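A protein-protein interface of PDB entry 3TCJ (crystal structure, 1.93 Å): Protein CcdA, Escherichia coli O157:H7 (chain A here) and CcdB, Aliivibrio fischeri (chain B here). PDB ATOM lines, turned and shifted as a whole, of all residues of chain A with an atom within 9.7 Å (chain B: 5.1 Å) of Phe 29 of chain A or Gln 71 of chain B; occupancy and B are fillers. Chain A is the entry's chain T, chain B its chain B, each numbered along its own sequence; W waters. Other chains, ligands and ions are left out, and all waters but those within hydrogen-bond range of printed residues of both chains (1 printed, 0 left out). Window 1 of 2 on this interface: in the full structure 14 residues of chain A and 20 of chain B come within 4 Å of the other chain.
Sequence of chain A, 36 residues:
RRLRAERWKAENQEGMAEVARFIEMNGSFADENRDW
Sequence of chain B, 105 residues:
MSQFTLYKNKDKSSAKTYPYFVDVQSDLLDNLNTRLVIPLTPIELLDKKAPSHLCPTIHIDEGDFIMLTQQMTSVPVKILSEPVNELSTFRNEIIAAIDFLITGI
OH of Tyr 18 of chain B lies within hydrogen-bond range of O of Gly 27 of chain A (2.7 Å). OE1 of Gln 71 of chain B sits at hydrogen-bond distance from N of Phe 29 of chain A (3.1 Å). The side-chain amide oxygen (OE1) of Gln 71 of chain B lies within hydrogen-bond range of the backbone NH (N) of Ala 30 of chain A, at 3.1 Å.
ND2 of Asn 9 of chain B sits at hydrogen-bond distance from OG of Ser 14 of chain B. The side-chain amide oxygen of Asn 33 of chain A lies close to the backbone carbonyl oxygen of Phe 29 of chain A. The backbone carbonyl oxygen (O) of Thr 73 of chain B is in hydrogen-bond range of the backbone NH (N) of Val 37 of chain B, 2.9 Å away. ND2 of Asn 9 of chain B lies within hydrogen-bond range of O of Tyr 18 of chain B, at 2.8 Å. NH2 of Arg 34 of chain A is in salt-bridge range of OD1 of Asp 31 of chain A (2.7 Å). The backbone NH (N) of Leu 68 of chain B lies within hydrogen-bond range of the backbone carbonyl oxygen (O) of Pro 39 of chain B, at 3.1 Å.
Val 19 of chain A touches Gln 70 of chain B. Gln 70 of chain B touches Ile 23 of chain A. CD1 of Ile 23 of chain A touches NE2 of Gln 71 of chain B (3.5 Å). Ser 28 of chain A touches Tyr 18 of chain B. ND2 of Asn 9 of chain B touches CE1 of Phe 29 of chain A (3.9 Å). CE2 of Tyr 18 of chain B touches N of Phe 29 of chain A (3.4 Å). Phe 29 of chain A touches Pro 39 of chain B. Ala 30 of chain A touches Thr 73 of chain B (CA to CG2, 3.9 Å). Val 75 of chain B touches Asn 33 of chain A. CA of Arg 34 of chain A touches OG1 of Thr 73 of chain B, at 3.8 Å.
Gln 71 of chain B touches just these residues of chain A: Ile 23 (3.5 Å), Ser 28 (3.4 Å), Phe 29 (3.1 Å) and Ala 30 (3.1 Å). Of the printed residues of chain A, Thr 73 of chain B touches Phe 29, Ala 30 and Arg 34. Printed residues of chain A within 4 Å of Ser 14 of chain B: Asn 33. Of the printed residues of chain A, Phe 21 of chain B touches Phe 29 (3.98 Å). Printed residues of chain B within 4 Å of Ile 23 of chain A: Gln 70 (3.6 Å) and Gln 71 (3.5 Å). Asn 26 of chain A touches none of the printed residues of chain B. The nearest residue of chain B that does not touch Phe 29 of chain A is Ser 14 of chain B (4.3 Å).
Hydrophobic or aromatic side chains of chain B that line the printed part of chain A: Tyr 18, Phe 21, Val 37, Pro 39 and Val 75. Printed residues of chain A that touch a printed residue of chain B: Val 19, Ile 23, Gly 27, Ser 28, Phe 29, Ala 30, Asn 33 and Arg 34. Hydrophobic or aromatic side chains of chain A that line the printed part of chain B: Val 19, Ile 23, Phe 29 and Ala 30.
Water W1 bridges the side-chain amide oxygen of Asn 9 of chain B and the side-chain amide nitrogen of Asn 33 of chain A.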
ATOM      1  N   VAL A  19     -11.518  -4.500  -5.989  1.00  0.00           N
ATOM      2  CA  VAL A  19     -11.269  -3.687  -7.173  1.00  0.00           C
ATOM      3  C   VAL A  19     -11.139  -4.557  -8.418  1.00  0.00           C
ATOM      4  O   VAL A  19     -11.707  -4.248  -9.465  1.00  0.00           O
ATOM      5  CB  VAL A  19      -9.993  -2.842  -7.018  1.00  0.00           C
ATOM      6  CG1 VAL A  19      -9.623  -2.190  -8.341  1.00  0.00           C
ATOM      7  CG2 VAL A  19     -10.180  -1.796  -5.931  1.00  0.00           C
ATOM      8  N   ALA A  20     -10.383  -5.644  -8.294  1.00  0.00           N
ATOM      9  CA  ALA A  20     -10.189  -6.577  -9.397  1.00  0.00           C
ATOM     10  C   ALA A  20     -11.521  -7.141  -9.888  1.00  0.00           C
ATOM     11  O   ALA A  20     -11.786  -7.165 -11.089  1.00  0.00           O
ATOM     12  CB  ALA A  20      -9.248  -7.701  -8.986  1.00  0.00           C
ATOM     13  N   PHE A  22     -14.315  -5.781  -9.522  1.00  0.00           N
ATOM     14  CA  PHE A  22     -15.054  -4.651 -10.069  1.00  0.00           C
ATOM     15  C   PHE A  22     -14.707  -4.423 -11.536  1.00  0.00           C
ATOM     16  O   PHE A  22     -15.586  -4.173 -12.361  1.00  0.00           O
ATOM     17  CB  PHE A  22     -14.775  -3.382  -9.263  1.00  0.00           C
ATOM     18  CG  PHE A  22     -15.196  -2.122  -9.961  1.00  0.00           C
ATOM     19  CD1 PHE A  22     -16.524  -1.739  -9.981  1.00  0.00           C
ATOM     20  CD2 PHE A  22     -14.263  -1.324 -10.604  1.00  0.00           C
ATOM     21  CE1 PHE A  22     -16.914  -0.583 -10.627  1.00  0.00           C
ATOM     22  CE2 PHE A  22     -14.646  -0.166 -11.251  1.00  0.00           C
ATOM     23  CZ  PHE A  22     -15.974   0.205 -11.262  1.00  0.00           C
ATOM     24  N   ILE A  23     -13.420  -4.510 -11.852  1.00  0.00           N
ATOM     25  CA  ILE A  23     -12.946  -4.302 -13.215  1.00  0.00           C
ATOM     26  C   ILE A  23     -13.337  -5.463 -14.130  1.00  0.00           C
ATOM     27  O   ILE A  23     -13.588  -5.270 -15.321  1.00  0.00           O
ATOM     28  CB  ILE A  23     -11.416  -4.098 -13.246  1.00  0.00           C
ATOM     29  CG1 ILE A  23     -11.036  -2.825 -12.483  1.00  0.00           C
ATOM     30  CG2 ILE A  23     -10.912  -4.029 -14.677  1.00  0.00           C
ATOM     31  CD1 ILE A  23      -9.551  -2.512 -12.510  1.00  0.00           C
ATOM     32  N   GLU A  24     -13.391  -6.665 -13.571  1.00  0.00           N
ATOM     33  CA  GLU A  24     -13.789  -7.842 -14.334  1.00  0.00           C
ATOM     34  C   GLU A  24     -15.271  -7.782 -14.684  1.00  0.00           C
ATOM     35  O   GLU A  24     -15.685  -8.218 -15.759  1.00  0.00           O
ATOM     36  CB  GLU A  24     -13.487  -9.119 -13.545  1.00  0.00           C
ATOM     37  CG  GLU A  24     -13.951 -10.395 -14.229  1.00  0.00           C
ATOM     38  N   ASN A  26     -17.074  -4.923 -14.770  1.00  0.00           N
ATOM     39  CA  ASN A  26     -17.431  -3.645 -15.382  1.00  0.00           C
ATOM     40  C   ASN A  26     -16.537  -3.242 -16.555  1.00  0.00           C
ATOM     41  O   ASN A  26     -16.749  -2.198 -17.173  1.00  0.00           O
ATOM     42  CB  ASN A  26     -17.458  -2.532 -14.330  1.00  0.00           C
ATOM     43  CG  ASN A  26     -18.475  -2.790 -13.232  1.00  0.00           C
ATOM     44  OD1 ASN A  26     -18.483  -3.854 -12.614  1.00  0.00           O
ATOM     45  ND2 ASN A  26     -19.333  -1.808 -12.980  1.00  0.00           N
ATOM     46  N   GLY A  27     -15.541  -4.069 -16.857  1.00  0.00           N
ATOM     47  CA  GLY A  27     -14.644  -3.807 -17.969  1.00  0.00           C
ATOM     48  C   GLY A  27     -13.433  -2.980 -17.581  1.00  0.00           C
ATOM     49  O   GLY A  27     -13.435  -2.307 -16.552  1.00  0.00           O
ATOM     50  N   SER A  28     -12.395  -3.032 -18.411  1.00  0.00           N
ATOM     51  CA  SER A  28     -11.160  -2.296 -18.152  1.00  0.00           C
ATOM     52  C   SER A  28     -10.985  -1.118 -19.109  1.00  0.00           C
ATOM     53  O   SER A  28     -11.106  -1.266 -20.325  1.00  0.00           O
ATOM     54  CB  SER A  28      -9.950  -3.228 -18.243  1.00  0.00           C
ATOM     55  N   PHE A  29     -10.693   0.051 -18.548  1.00  0.00           N
ATOM     56  CA  PHE A  29     -10.479   1.254 -19.341  1.00  0.00           C
ATOM     57  C   PHE A  29      -9.258   1.124 -20.250  1.00  0.00           C
ATOM     58  O   PHE A  29      -9.320   1.446 -21.437  1.00  0.00           O
ATOM     59  CB  PHE A  29     -10.327   2.470 -18.425  1.00  0.00           C
ATOM     60  CG  PHE A  29     -10.065   3.754 -19.158  1.00  0.00           C
ATOM     61  CD1 PHE A  29     -11.110   4.481 -19.704  1.00  0.00           C
ATOM     62  CD2 PHE A  29      -8.775   4.239 -19.295  1.00  0.00           C
ATOM     63  CE1 PHE A  29     -10.872   5.662 -20.378  1.00  0.00           C
ATOM     64  CE2 PHE A  29      -8.530   5.420 -19.969  1.00  0.00           C
ATOM     65  CZ  PHE A  29      -9.579   6.134 -20.510  1.00  0.00           C
ATOM     66  N   ALA A  30      -8.153   0.647 -19.685  1.00  0.00           N
ATOM     67  CA  ALA A  30      -6.893   0.535 -20.417  1.00  0.00           C
ATOM     68  C   ALA A  30      -7.026  -0.301 -21.687  1.00  0.00           C
ATOM     69  O   ALA A  30      -6.652   0.136 -22.773  1.00  0.00           O
ATOM     70  CB  ALA A  30      -5.809  -0.040 -19.516  1.00  0.00           C
ATOM     71  N   ASP A  31      -7.563  -1.507 -21.539  1.00  0.00           N
ATOM     72  CA  ASP A  31      -7.702  -2.435 -22.656  1.00  0.00           C
ATOM     73  C   ASP A  31      -8.519  -1.855 -23.809  1.00  0.00           C
ATOM     74  O   ASP A  31      -8.270  -2.164 -24.974  1.00  0.00           O
ATOM     75  CB  ASP A  31      -8.339  -3.743 -22.180  1.00  0.00           C
ATOM     76  CG  ASP A  31      -7.508  -4.442 -21.123  1.00  0.00           C
ATOM     77  OD1 ASP A  31      -6.321  -4.092 -20.970  1.00  0.00           O
ATOM     78  OD2 ASP A  31      -8.044  -5.345 -20.446  1.00  0.00           O
ATOM     79  N   GLU A  32      -9.491  -1.011 -23.480  1.00  0.00           N
ATOM     80  CA  GLU A  32     -10.409  -0.484 -24.485  1.00  0.00           C
ATOM     81  C   GLU A  32      -9.910   0.811 -25.132  1.00  0.00           C
ATOM     82  O   GLU A  32     -10.431   1.232 -26.166  1.00  0.00           O
ATOM     83  CB  GLU A  32     -11.800  -0.273 -23.881  1.00  0.00           C
ATOM     84  N   ASN A  33      -8.899   1.429 -24.527  1.00  0.00           N
ATOM     85  CA  ASN A  33      -8.389   2.716 -25.001  1.00  0.00           C
ATOM     86  C   ASN A  33      -6.896   2.712 -25.320  1.00  0.00           C
ATOM     87  O   ASN A  33      -6.367   3.687 -25.855  1.00  0.00           O
ATOM     88  CB  ASN A  33      -8.686   3.811 -23.978  1.00  0.00           C
ATOM     89  CG  ASN A  33     -10.164   4.123 -23.872  1.00  0.00           C
ATOM     90  OD1 ASN A  33     -10.841   3.668 -22.950  1.00  0.00           O
ATOM     91  ND2 ASN A  33     -10.674   4.897 -24.822  1.00  0.00           N
ATOM     92  N   ARG A  34      -6.221   1.620 -24.982  1.00  0.00           N
ATOM     93  CA  ARG A  34      -4.787   1.496 -25.223  1.00  0.00           C
ATOM     94  C   ARG A  34      -4.419   1.759 -26.682  1.00  0.00           C
ATOM     95  O   ARG A  34      -5.132   1.346 -27.598  1.00  0.00           O
ATOM     96  CB  ARG A  34      -4.290   0.119 -24.783  1.00  0.00           C
ATOM     97  CG  ARG A  34      -3.104  -0.406 -25.566  1.00  0.00           C
ATOM     98  CD  ARG A  34      -2.211  -1.264 -24.688  1.00  0.00           C
ATOM     99  NE  ARG A  34      -2.858  -1.621 -23.428  1.00  0.00           N
ATOM    100  CZ  ARG A  34      -3.621  -2.694 -23.251  1.00  0.00           C
ATOM    101  NH1 ARG A  34      -3.848  -3.528 -24.256  1.00  0.00           N
ATOM    102  NH2 ARG A  34      -4.164  -2.931 -22.064  1.00  0.00           N
ATOM    103  N   ASP A  35      -3.300   2.448 -26.885  1.00  0.00           N
ATOM    104  CA  ASP A  35      -2.864   2.837 -28.221  1.00  0.00           C
ATOM    105  C   ASP A  35      -1.778   1.918 -28.789  1.00  0.00           C
ATOM    106  O   ASP A  35      -0.754   2.394 -29.282  1.00  0.00           O
ATOM    107  CB  ASP A  35      -2.371   4.287 -28.215  1.00  0.00           C
ATOM    108  N   ASN B   9     -15.412  10.947 -21.246  1.00  0.00           N
ATOM    109  CA  ASN B   9     -15.106   9.755 -22.024  1.00  0.00           C
ATOM    110  C   ASN B   9     -16.078   9.583 -23.183  1.00  0.00           C
ATOM    111  O   ASN B   9     -17.276   9.396 -22.976  1.00  0.00           O
ATOM    112  CB  ASN B   9     -15.136   8.517 -21.127  1.00  0.00           C
ATOM    113  CG  ASN B   9     -14.698   7.259 -21.849  1.00  0.00           C
ATOM    114  OD1 ASN B   9     -14.401   7.285 -23.043  1.00  0.00           O
ATOM    115  ND2 ASN B   9     -14.658   6.147 -21.125  1.00  0.00           N
ATOM    116  N   SER B  14     -16.927   2.117 -22.745  1.00  0.00           N
ATOM    117  CA  SER B  14     -16.320   2.285 -21.428  1.00  0.00           C
ATOM    118  C   SER B  14     -16.835   3.522 -20.696  1.00  0.00           C
ATOM    119  O   SER B  14     -16.461   3.769 -19.549  1.00  0.00           O
ATOM    120  CB  SER B  14     -14.795   2.346 -21.549  1.00  0.00           C
ATOM    121  OG  SER B  14     -14.385   3.490 -22.279  1.00  0.00           O
ATOM    122  N   TYR B  18     -16.439   4.401 -16.812  1.00  0.00           N
ATOM    123  CA  TYR B  18     -15.407   5.429 -16.770  1.00  0.00           C
ATOM    124  C   TYR B  18     -15.858   6.697 -17.491  1.00  0.00           C
ATOM    125  O   TYR B  18     -15.419   6.969 -18.605  1.00  0.00           O
ATOM    126  CB  TYR B  18     -14.115   4.906 -17.402  1.00  0.00           C
ATOM    127  CG  TYR B  18     -13.664   3.570 -16.856  1.00  0.00           C
ATOM    128  CD1 TYR B  18     -12.991   3.484 -15.645  1.00  0.00           C
ATOM    129  CD2 TYR B  18     -13.909   2.393 -17.553  1.00  0.00           C
ATOM    130  CE1 TYR B  18     -12.576   2.267 -15.142  1.00  0.00           C
ATOM    131  CE2 TYR B  18     -13.497   1.170 -17.058  1.00  0.00           C
ATOM    132  CZ  TYR B  18     -12.830   1.114 -15.851  1.00  0.00           C
ATOM    133  OH  TYR B  18     -12.415  -0.097 -15.348  1.00  0.00           O
ATOM    134  N   PHE B  21     -11.762  10.910 -17.651  1.00  0.00           N
ATOM    135  CA  PHE B  21     -10.361  10.583 -17.422  1.00  0.00           C
ATOM    136  C   PHE B  21      -9.532  11.862 -17.357  1.00  0.00           C
ATOM    137  O   PHE B  21      -9.884  12.874 -17.965  1.00  0.00           O
ATOM    138  CB  PHE B  21      -9.830   9.633 -18.500  1.00  0.00           C
ATOM    139  CG  PHE B  21      -9.884  10.190 -19.895  1.00  0.00           C
ATOM    140  CD1 PHE B  21      -8.881  11.022 -20.363  1.00  0.00           C
ATOM    141  CD2 PHE B  21     -10.930   9.867 -20.745  1.00  0.00           C
ATOM    142  CE1 PHE B  21      -8.924  11.529 -21.649  1.00  0.00           C
ATOM    143  CE2 PHE B  21     -10.979  10.372 -22.033  1.00  0.00           C
ATOM    144  CZ  PHE B  21      -9.972  11.203 -22.485  1.00  0.00           C
ATOM    145  N   VAL B  37      -3.113   9.049 -19.465  1.00  0.00           N
ATOM    146  CA  VAL B  37      -4.324   9.444 -18.754  1.00  0.00           C
ATOM    147  C   VAL B  37      -4.743   8.413 -17.712  1.00  0.00           C
ATOM    148  O   VAL B  37      -4.354   7.246 -17.783  1.00  0.00           O
ATOM    149  CB  VAL B  37      -5.503   9.691 -19.727  1.00  0.00           C
ATOM    150  CG1 VAL B  37      -5.119  10.718 -20.784  1.00  0.00           C
ATOM    151  CG2 VAL B  37      -5.941   8.389 -20.380  1.00  0.00           C
ATOM    152  N   PRO B  39      -8.321   7.011 -15.702  1.00  0.00           N
ATOM    153  CA  PRO B  39      -9.786   7.063 -15.727  1.00  0.00           C
ATOM    154  C   PRO B  39     -10.401   7.265 -14.344  1.00  0.00           C
ATOM    155  O   PRO B  39      -9.803   6.895 -13.332  1.00  0.00           O
ATOM    156  CB  PRO B  39     -10.170   5.688 -16.277  1.00  0.00           C
ATOM    157  CG  PRO B  39      -9.047   4.793 -15.888  1.00  0.00           C
ATOM    158  CD  PRO B  39      -7.804   5.633 -15.783  1.00  0.00           C
ATOM    159  N   LEU B  68      -8.737   5.426 -10.793  1.00  0.00           N
ATOM    160  CA  LEU B  68      -8.177   4.086 -10.928  1.00  0.00           C
ATOM    161  C   LEU B  68      -6.776   4.123 -11.532  1.00  0.00           C
ATOM    162  O   LEU B  68      -6.589   3.835 -12.713  1.00  0.00           O
ATOM    163  CB  LEU B  68      -9.103   3.199 -11.766  1.00  0.00           C
ATOM    164  CG  LEU B  68     -10.438   2.849 -11.104  1.00  0.00           C
ATOM    165  CD1 LEU B  68     -11.299   2.003 -12.028  1.00  0.00           C
ATOM    166  CD2 LEU B  68     -10.214   2.139  -9.777  1.00  0.00           C
ATOM    167  N   THR B  69      -5.800   4.474 -10.703  1.00  0.00           N
ATOM    168  CA  THR B  69      -4.413   4.600 -11.137  1.00  0.00           C
ATOM    169  C   THR B  69      -3.903   3.324 -11.798  1.00  0.00           C
ATOM    170  O   THR B  69      -3.087   3.373 -12.719  1.00  0.00           O
ATOM    171  CB  THR B  69      -3.496   4.949  -9.949  1.00  0.00           C
ATOM    172  OG1 THR B  69      -4.109   5.975  -9.161  1.00  0.00           O
ATOM    173  CG2 THR B  69      -2.135   5.426 -10.438  1.00  0.00           C
ATOM    174  N   GLN B  70      -4.390   2.181 -11.327  1.00  0.00           N
ATOM    175  CA  GLN B  70      -3.955   0.891 -11.850  1.00  0.00           C
ATOM    176  C   GLN B  70      -4.442   0.666 -13.283  1.00  0.00           C
ATOM    177  O   GLN B  70      -4.032  -0.286 -13.944  1.00  0.00           O
ATOM    178  CB  GLN B  70      -4.436  -0.244 -10.940  1.00  0.00           C
ATOM    179  CG  GLN B  70      -5.934  -0.489 -10.985  1.00  0.00           C
ATOM    180  CD  GLN B  70      -6.437  -1.252  -9.773  1.00  0.00           C
ATOM    181  OE1 GLN B  70      -6.371  -0.763  -8.645  1.00  0.00           O
ATOM    182  NE2 GLN B  70      -6.948  -2.457 -10.001  1.00  0.00           N
ATOM    183  N   GLN B  71      -5.319   1.547 -13.756  1.00  0.00           N
ATOM    184  CA  GLN B  71      -5.830   1.467 -15.121  1.00  0.00           C
ATOM    185  C   GLN B  71      -5.266   2.589 -15.989  1.00  0.00           C
ATOM    186  O   GLN B  71      -5.793   2.885 -17.061  1.00  0.00           O
ATOM    187  CB  GLN B  71      -7.360   1.509 -15.123  1.00  0.00           C
ATOM    188  CG  GLN B  71      -8.017   0.213 -14.679  1.00  0.00           C
ATOM    189  CD  GLN B  71      -7.885  -0.890 -15.714  1.00  0.00           C
ATOM    190  OE1 GLN B  71      -8.193  -0.694 -16.891  1.00  0.00           O
ATOM    191  NE2 GLN B  71      -7.430  -2.059 -15.278  1.00  0.00           N
ATOM    192  N   MET B  72      -4.194   3.216 -15.512  1.00  0.00           N
ATOM    193  CA  MET B  72      -3.533   4.281 -16.255  1.00  0.00           C
ATOM    194  C   MET B  72      -3.076   3.757 -17.611  1.00  0.00           C
ATOM    195  O   MET B  72      -2.614   2.621 -17.718  1.00  0.00           O
ATOM    196  CB  MET B  72      -2.337   4.809 -15.460  1.00  0.00           C
ATOM    197  CG  MET B  72      -1.653   6.016 -16.074  1.00  0.00           C
ATOM    198  SD  MET B  72      -0.413   6.719 -14.970  1.00  0.00           S
ATOM    199  CE  MET B  72       0.650   5.299 -14.718  1.00  0.00           C
ATOM    200  N   THR B  73      -3.209   4.576 -18.649  1.00  0.00           N
ATOM    201  CA  THR B  73      -2.850   4.136 -19.992  1.00  0.00           C
ATOM    202  C   THR B  73      -2.546   5.286 -20.945  1.00  0.00           C
ATOM    203  O   THR B  73      -3.021   6.406 -20.762  1.00  0.00           O
ATOM    204  CB  THR B  73      -3.963   3.269 -20.615  1.00  0.00           C
ATOM    205  OG1 THR B  73      -3.531   2.770 -21.887  1.00  0.00           O
ATOM    206  CG2 THR B  73      -5.233   4.085 -20.800  1.00  0.00           C
ATOM    207  N   VAL B  75      -3.064   7.011 -24.497  1.00  0.00           N
ATOM    208  CA  VAL B  75      -4.126   7.073 -25.491  1.00  0.00           C
ATOM    209  C   VAL B  75      -3.768   8.074 -26.579  1.00  0.00           C
ATOM    210  O   VAL B  75      -2.993   9.000 -26.344  1.00  0.00           O
ATOM    211  CB  VAL B  75      -5.464   7.492 -24.856  1.00  0.00           C
ATOM    212  CG1 VAL B  75      -5.862   6.516 -23.755  1.00  0.00           C
ATOM    213  CG2 VAL B  75      -5.375   8.912 -24.314  1.00  0.00           C
HETATM  214  O   HOH W   1     -12.012   7.552 -24.246  1.00  0.00           O
